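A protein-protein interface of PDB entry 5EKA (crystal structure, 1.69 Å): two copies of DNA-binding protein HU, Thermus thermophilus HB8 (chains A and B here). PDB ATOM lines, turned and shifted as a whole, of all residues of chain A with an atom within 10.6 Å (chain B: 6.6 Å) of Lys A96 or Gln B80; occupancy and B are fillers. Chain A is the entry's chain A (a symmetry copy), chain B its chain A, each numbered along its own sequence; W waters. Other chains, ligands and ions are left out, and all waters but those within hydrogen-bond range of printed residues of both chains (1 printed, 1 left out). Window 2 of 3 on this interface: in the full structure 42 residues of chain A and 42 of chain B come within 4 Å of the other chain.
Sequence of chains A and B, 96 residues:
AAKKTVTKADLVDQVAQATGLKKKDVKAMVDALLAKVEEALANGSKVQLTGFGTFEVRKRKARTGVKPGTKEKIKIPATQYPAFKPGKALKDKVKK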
ATOM      1  N   ALA A   1     -21.389 -14.847  13.022  1.00  0.00           N
ATOM      2  CA  ALA A   1     -22.743 -15.019  12.430  1.00  0.00           C
ATOM      3  C   ALA A   1     -23.577 -15.857  13.380  1.00  0.00           C
ATOM      4  O   ALA A   1     -23.034 -16.748  14.073  1.00  0.00           O
ATOM      5  CB  ALA A   1     -22.666 -15.674  11.062  1.00  0.00           C
ATOM      6  N   PRO A  86     -16.615 -10.412  -7.298  1.00  0.00           N
ATOM      7  CA  PRO A  86     -17.848  -9.880  -6.738  1.00  0.00           C
ATOM      8  C   PRO A  86     -18.169  -8.507  -7.283  1.00  0.00           C
ATOM      9  O   PRO A  86     -17.260  -7.725  -7.542  1.00  0.00           O
ATOM     10  CB  PRO A  86     -17.548  -9.774  -5.241  1.00  0.00           C
ATOM     11  CG  PRO A  86     -16.115  -9.731  -5.132  1.00  0.00           C
ATOM     12  CD  PRO A  86     -15.563 -10.528  -6.287  1.00  0.00           C
ATOM     13  N   GLY A  87     -19.452  -8.266  -7.474  1.00  0.00           N
ATOM     14  CA  GLY A  87     -19.932  -6.990  -7.910  1.00  0.00           C
ATOM     15  C   GLY A  87     -19.931  -5.958  -6.827  1.00  0.00           C
ATOM     16  O   GLY A  87     -19.799  -6.262  -5.646  1.00  0.00           O
ATOM     17  N   LYS A  88     -20.110  -4.707  -7.238  1.00  0.00           N
ATOM     18  CA  LYS A  88     -20.077  -3.622  -6.283  1.00  0.00           C
ATOM     19  C   LYS A  88     -21.126  -3.705  -5.188  1.00  0.00           C
ATOM     20  O   LYS A  88     -20.843  -3.426  -4.007  1.00  0.00           O
ATOM     21  CB  LYS A  88     -20.246  -2.294  -6.998  1.00  0.00           C
ATOM     22  CG  LYS A  88     -20.178  -1.122  -6.037  1.00  0.00           C
ATOM     23  CD  LYS A  88     -20.112   0.166  -6.794  1.00  0.00           C
ATOM     24  CE  LYS A  88     -19.702   1.344  -5.918  1.00  0.00           C
ATOM     25  NZ  LYS A  88     -20.737   1.695  -4.908  1.00  0.00           N
ATOM     26  N   ALA A  89     -22.349  -4.044  -5.569  1.00  0.00           N
ATOM     27  CA  ALA A  89     -23.422  -4.156  -4.574  1.00  0.00           C
ATOM     28  C   ALA A  89     -23.087  -5.154  -3.466  1.00  0.00           C
ATOM     29  O   ALA A  89     -23.313  -4.891  -2.280  1.00  0.00           O
ATOM     30  CB  ALA A  89     -24.727  -4.524  -5.244  1.00  0.00           C
ATOM     31  N   LEU A  90     -22.542  -6.290  -3.867  1.00  0.00           N
ATOM     32  CA  LEU A  90     -22.177  -7.339  -2.919  1.00  0.00           C
ATOM     33  C   LEU A  90     -20.994  -6.873  -2.066  1.00  0.00           C
ATOM     34  O   LEU A  90     -21.002  -7.028  -0.845  1.00  0.00           O
ATOM     35  CB  LEU A  90     -21.870  -8.625  -3.663  1.00  0.00           C
ATOM     36  CG  LEU A  90     -21.500  -9.784  -2.734  1.00  0.00           C
ATOM     37  CD1 LEU A  90     -22.598 -10.119  -1.748  1.00  0.00           C
ATOM     38  CD2 LEU A  90     -21.045 -11.004  -3.515  1.00  0.00           C
ATOM     39  N   LYS A  91     -19.999  -6.228  -2.692  1.00  0.00           N
ATOM     40  CA  LYS A  91     -18.842  -5.730  -1.949  1.00  0.00           C
ATOM     41  C   LYS A  91     -19.310  -4.728  -0.896  1.00  0.00           C
ATOM     42  O   LYS A  91     -18.849  -4.738   0.229  1.00  0.00           O
ATOM     43  CB  LYS A  91     -17.823  -5.109  -2.898  1.00  0.00           C
ATOM     44  CG  LYS A  91     -17.031  -6.154  -3.683  1.00  0.00           C
ATOM     45  CD  LYS A  91     -15.923  -5.512  -4.442  1.00  0.00           C
ATOM     46  CE  LYS A  91     -16.398  -4.807  -5.686  1.00  0.00           C
ATOM     47  NZ  LYS A  91     -15.245  -4.240  -6.444  1.00  0.00           N
ATOM     48  N   ASP A  92     -20.251  -3.872  -1.274  1.00  0.00           N
ATOM     49  CA  ASP A  92     -20.738  -2.840  -0.370  1.00  0.00           C
ATOM     50  C   ASP A  92     -21.517  -3.429   0.814  1.00  0.00           C
ATOM     51  O   ASP A  92     -21.380  -2.971   1.958  1.00  0.00           O
ATOM     52  CB  ASP A  92     -21.587  -1.828  -1.173  1.00  0.00           C
ATOM     53  CG  ASP A  92     -20.716  -0.888  -2.047  1.00  0.00           C
ATOM     54  OD1 ASP A  92     -19.461  -0.737  -1.805  1.00  0.00           O
ATOM     55  OD2 ASP A  92     -21.288  -0.224  -2.948  1.00  0.00           O
ATOM     56  N   LYS A  93     -22.320  -4.453   0.539  1.00  0.00           N
ATOM     57  CA  LYS A  93     -23.136  -5.096   1.591  1.00  0.00           C
ATOM     58  C   LYS A  93     -22.298  -5.861   2.621  1.00  0.00           C
ATOM     59  O   LYS A  93     -22.750  -6.071   3.758  1.00  0.00           O
ATOM     60  CB  LYS A  93     -24.184  -6.048   0.993  1.00  0.00           C
ATOM     61  CG  LYS A  93     -25.416  -5.306   0.514  1.00  0.00           C
ATOM     62  CD  LYS A  93     -26.681  -6.116   0.702  1.00  0.00           C
ATOM     63  CE  LYS A  93     -27.162  -6.189   2.148  1.00  0.00           C
ATOM     64  NZ  LYS A  93     -27.835  -7.503   2.412  1.00  0.00           N
ATOM     65  N   VAL A  94     -21.085  -6.262   2.246  1.00  0.00           N
ATOM     66  CA  VAL A  94     -20.245  -7.076   3.148  1.00  0.00           C
ATOM     67  C   VAL A  94     -19.289  -6.235   3.998  1.00  0.00           C
ATOM     68  O   VAL A  94     -18.737  -6.718   4.976  1.00  0.00           O
ATOM     69  CB  VAL A  94     -19.488  -8.137   2.337  1.00  0.00           C
ATOM     70  CG1 VAL A  94     -18.351  -8.802   3.102  1.00  0.00           C
ATOM     71  CG2 VAL A  94     -20.501  -9.175   1.881  1.00  0.00           C
ATOM     72  N   LYS A  95     -19.134  -4.965   3.658  1.00  0.00           N
ATOM     73  CA  LYS A  95     -18.394  -4.062   4.524  1.00  0.00           C
ATOM     74  C   LYS A  95     -19.052  -3.927   5.893  1.00  0.00           C
ATOM     75  O   LYS A  95     -20.267  -3.987   6.030  1.00  0.00           O
ATOM     76  CB  LYS A  95     -18.266  -2.688   3.874  1.00  0.00           C
ATOM     77  CG  LYS A  95     -17.432  -2.734   2.615  1.00  0.00           C
ATOM     78  CD  LYS A  95     -17.340  -1.384   1.955  1.00  0.00           C
ATOM     79  CE  LYS A  95     -16.604  -1.476   0.627  1.00  0.00           C
ATOM     80  NZ  LYS A  95     -15.941  -0.175   0.320  1.00  0.00           N
ATOM     81  N   LYS A  96     -18.246  -3.749   6.923  1.00  0.00           N
ATOM     82  CA  LYS A  96     -18.817  -3.493   8.235  1.00  0.00           C
ATOM     83  C   LYS A  96     -19.358  -2.065   8.278  1.00  0.00           C
ATOM     84  O   LYS A  96     -18.815  -1.172   7.619  1.00  0.00           O
ATOM     85  CB  LYS A  96     -17.804  -3.761   9.354  1.00  0.00           C
ATOM     86  CG  LYS A  96     -18.080  -5.059  10.113  1.00  0.00           C
ATOM     87  CD  LYS A  96     -19.305  -4.918  11.018  1.00  0.00           C
ATOM     88  CE  LYS A  96     -19.611  -6.195  11.784  1.00  0.00           C
ATOM     89  NZ  LYS A  96     -20.309  -5.913  13.076  1.00  0.00           N
ATOM     90  OXT LYS A  96     -20.366  -1.785   8.941  1.00  0.00           O
ATOM     91  N   LEU B  41     -23.823 -13.659   3.685  1.00  0.00           N
ATOM     92  CA  LEU B  41     -22.495 -13.063   3.696  1.00  0.00           C
ATOM     93  C   LEU B  41     -22.410 -11.764   4.516  1.00  0.00           C
ATOM     94  O   LEU B  41     -21.440 -11.538   5.247  1.00  0.00           O
ATOM     95  CB  LEU B  41     -22.003 -12.855   2.268  1.00  0.00           C
ATOM     96  CG  LEU B  41     -21.719 -14.149   1.493  1.00  0.00           C
ATOM     97  CD1 LEU B  41     -21.471 -13.827   0.039  1.00  0.00           C
ATOM     98  CD2 LEU B  41     -20.564 -14.943   2.090  1.00  0.00           C
ATOM     99  N   ALA B  42     -23.471 -10.970   4.453  1.00  0.00           N
ATOM    100  CA  ALA B  42     -23.537  -9.726   5.245  1.00  0.00           C
ATOM    101  C   ALA B  42     -23.510 -10.024   6.760  1.00  0.00           C
ATOM    102  O   ALA B  42     -22.975  -9.239   7.546  1.00  0.00           O
ATOM    103  CB  ALA B  42     -24.764  -8.924   4.857  1.00  0.00           C
ATOM    104  N   VAL B  57     -16.672 -14.308   3.729  1.00  0.00           N
ATOM    105  CA  VAL B  57     -16.127 -12.965   3.900  1.00  0.00           C
ATOM    106  C   VAL B  57     -14.713 -13.074   4.411  1.00  0.00           C
ATOM    107  O   VAL B  57     -14.467 -13.665   5.481  1.00  0.00           O
ATOM    108  CB  VAL B  57     -16.981 -12.183   4.910  1.00  0.00           C
ATOM    109  CG1 VAL B  57     -16.380 -10.799   5.174  1.00  0.00           C
ATOM    110  CG2 VAL B  57     -18.395 -12.081   4.390  1.00  0.00           C
ATOM    111  N   ARG B  58     -13.779 -12.494   3.670  1.00  0.00           N
ATOM    112  CA  ARG B  58     -12.378 -12.520   4.074  1.00  0.00           C
ATOM    113  C   ARG B  58     -11.987 -11.198   4.640  1.00  0.00           C
ATOM    114  O   ARG B  58     -12.593 -10.187   4.304  1.00  0.00           O
ATOM    115  CB  ARG B  58     -11.515 -12.902   2.897  1.00  0.00           C
ATOM    116  CG  ARG B  58     -11.771 -14.337   2.514  1.00  0.00           C
ATOM    117  CD  ARG B  58     -10.776 -14.854   1.489  1.00  0.00           C
ATOM    118  NE  ARG B  58     -11.258 -16.133   0.953  1.00  0.00           N
ATOM    119  CZ  ARG B  58     -10.890 -16.686  -0.204  1.00  0.00           C
ATOM    120  NH1 ARG B  58     -10.022 -16.088  -1.019  1.00  0.00           N
ATOM    121  NH2 ARG B  58     -11.426 -17.846  -0.559  1.00  0.00           N
ATOM    122  N   LYS B  59     -11.012 -11.210   5.543  1.00  0.00           N
ATOM    123  CA  LYS B  59     -10.556  -9.981   6.169  1.00  0.00           C
ATOM    124  C   LYS B  59      -9.115  -9.592   5.793  1.00  0.00           C
ATOM    125  O   LYS B  59      -8.258 -10.434   5.518  1.00  0.00           O
ATOM    126  CB  LYS B  59     -10.728 -10.093   7.679  1.00  0.00           C
ATOM    127  CG  LYS B  59     -12.178 -10.089   8.113  1.00  0.00           C
ATOM    128  CD  LYS B  59     -12.373 -10.397   9.590  1.00  0.00           C
ATOM    129  CE  LYS B  59     -13.634 -11.224   9.836  1.00  0.00           C
ATOM    130  NZ  LYS B  59     -14.899 -10.579   9.374  1.00  0.00           N
ATOM    131  N   ARG B  60      -8.891  -8.291   5.703  1.00  0.00           N
ATOM    132  CA  ARG B  60      -7.557  -7.764   5.607  1.00  0.00           C
ATOM    133  C   ARG B  60      -7.338  -6.977   6.903  1.00  0.00           C
ATOM    134  O   ARG B  60      -8.118  -6.103   7.223  1.00  0.00           O
ATOM    135  CB  ARG B  60      -7.431  -6.837   4.396  1.00  0.00           C
ATOM    136  CG  ARG B  60      -8.109  -7.321   3.110  1.00  0.00           C
ATOM    137  CD  ARG B  60      -7.706  -6.432   1.932  1.00  0.00           C
ATOM    138  NE  ARG B  60      -8.356  -6.773   0.659  1.00  0.00           N
ATOM    139  CZ  ARG B  60      -9.504  -6.261   0.210  1.00  0.00           C
ATOM    140  NH1 ARG B  60     -10.199  -5.380   0.930  1.00  0.00           N
ATOM    141  NH2 ARG B  60      -9.978  -6.658  -0.971  1.00  0.00           N
ATOM    142  N   ALA B  78      -8.466  -1.790   8.400  1.00  0.00           N
ATOM    143  CA  ALA B  78      -8.926  -3.160   8.180  1.00  0.00           C
ATOM    144  C   ALA B  78     -10.125  -3.118   7.233  1.00  0.00           C
ATOM    145  O   ALA B  78     -10.918  -2.182   7.272  1.00  0.00           O
ATOM    146  CB  ALA B  78      -9.305  -3.813   9.495  1.00  0.00           C
ATOM    147  N   THR B  79     -10.222  -4.116   6.366  1.00  0.00           N
ATOM    148  CA  THR B  79     -11.302  -4.182   5.397  1.00  0.00           C
ATOM    149  C   THR B  79     -11.769  -5.621   5.310  1.00  0.00           C
ATOM    150  O   THR B  79     -11.132  -6.518   5.796  1.00  0.00           O
ATOM    151  CB  THR B  79     -10.885  -3.722   3.989  1.00  0.00           C
ATOM    152  OG1 THR B  79      -9.678  -4.363   3.630  1.00  0.00           O
ATOM    153  CG2 THR B  79     -10.670  -2.206   3.942  1.00  0.00           C
ATOM    154  N   GLN B  80     -12.944  -5.816   4.740  1.00  0.00           N
ATOM    155  CA  GLN B  80     -13.436  -7.178   4.560  1.00  0.00           C
ATOM    156  C   GLN B  80     -14.188  -7.239   3.267  1.00  0.00           C
ATOM    157  O   GLN B  80     -14.741  -6.241   2.829  1.00  0.00           O
ATOM    158  CB  GLN B  80     -14.272  -7.642   5.750  1.00  0.00           C
ATOM    159  CG  GLN B  80     -15.539  -6.872   6.013  1.00  0.00           C
ATOM    160  CD  GLN B  80     -16.216  -7.265   7.336  1.00  0.00           C
ATOM    161  OE1 GLN B  80     -15.562  -7.441   8.368  1.00  0.00           O
ATOM    162  NE2 GLN B  80     -17.532  -7.387   7.308  1.00  0.00           N
ATOM    163  N   TYR B  81     -14.171  -8.407   2.651  1.00  0.00           N
ATOM    164  CA  TYR B  81     -14.632  -8.523   1.288  1.00  0.00           C
ATOM    165  C   TYR B  81     -15.136  -9.931   0.995  1.00  0.00           C
ATOM    166  O   TYR B  81     -14.763 -10.889   1.682  1.00  0.00           O
ATOM    167  CB  TYR B  81     -13.520  -8.141   0.326  1.00  0.00           C
ATOM    168  CG  TYR B  81     -12.296  -9.041   0.399  1.00  0.00           C
ATOM    169  CD1 TYR B  81     -12.148 -10.095  -0.482  1.00  0.00           C
ATOM    170  CD2 TYR B  81     -11.326  -8.870   1.375  1.00  0.00           C
ATOM    171  CE1 TYR B  81     -11.045 -10.929  -0.420  1.00  0.00           C
ATOM    172  CE2 TYR B  81     -10.214  -9.712   1.435  1.00  0.00           C
ATOM    173  CZ  TYR B  81     -10.101 -10.745   0.548  1.00  0.00           C
ATOM    174  OH  TYR B  81      -9.005 -11.592   0.598  1.00  0.00           O
ATOM    175  N   PRO B  82     -16.033 -10.039   0.008  1.00  0.00           N
ATOM    176  CA  PRO B  82     -16.550 -11.364  -0.299  1.00  0.00           C
ATOM    177  C   PRO B  82     -15.593 -12.126  -1.202  1.00  0.00           C
ATOM    178  O   PRO B  82     -14.989 -11.531  -2.082  1.00  0.00           O
ATOM    179  CB  PRO B  82     -17.870 -11.056  -1.036  1.00  0.00           C
ATOM    180  CG  PRO B  82     -17.767  -9.651  -1.554  1.00  0.00           C
ATOM    181  CD  PRO B  82     -16.592  -8.989  -0.880  1.00  0.00           C
HETATM  182  O   HOH W   1     -16.346  -5.713   0.511  1.00  0.00           O
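Printed residues of chain A that touch a printed residue of chain B: Pro A86, Leu A90, Lys A93, Val A94 and Lys A96. Hydrophobic or aromatic side chains of chain A that line the printed part of chain B: Pro A86, Leu A90 and Val A94. Printed residues of chain B that touch a printed residue of chain A: Leu B41, Ala B42, Val B57, Gln B80 and Pro B82. Among the printed residues, 7 pairs touch across the chains.
No position is printed for both chains. Of the 7 pairs that touch across the chains among the printed residues, none has its exchanged pair printed and touching as well.
O of Val A94 lies within hydrogen-bond range of NE2 of Gln B80, 2.7 Å away.
The side-chain amino group (NZ) of Lys B59 is in hydrogen-bond range of the side-chain amide oxygen (OE1) of Gln B80, at 3.4 Å.
Among the printed residues, merely in contact across the chains: Val A94 with Val B57 (3.5 Å), Lys A93 with Ala B42 (3.7 Å), Lys A96 with Gln B80 (3.7 Å), Pro A86 with Pro B82 (3.7 Å), Leu A90 with Pro B82 (3.9 Å) and Val A94 with Leu B41 (3.99 Å).
Of the printed residues of chain B, Pro A86 touches Pro B82 (3.7 Å). Of the printed residues of chain B, Leu A90 touches Pro B82 (3.9 Å). Lys A96 touches one residue of chain B. No residue of chain A comes within 4 Å of Thr B79. Tyr B81 touches none of the printed residues of chain A. The nearest residue of chain A that does not touch Gln B80 is Lys A95 (4.04 Å). The nearest printed residue of chain B that does not touch Pro A86 is Tyr B81 (6.1 Å).
Water W1 bridges O of Lys A91 and O of Gln B80.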
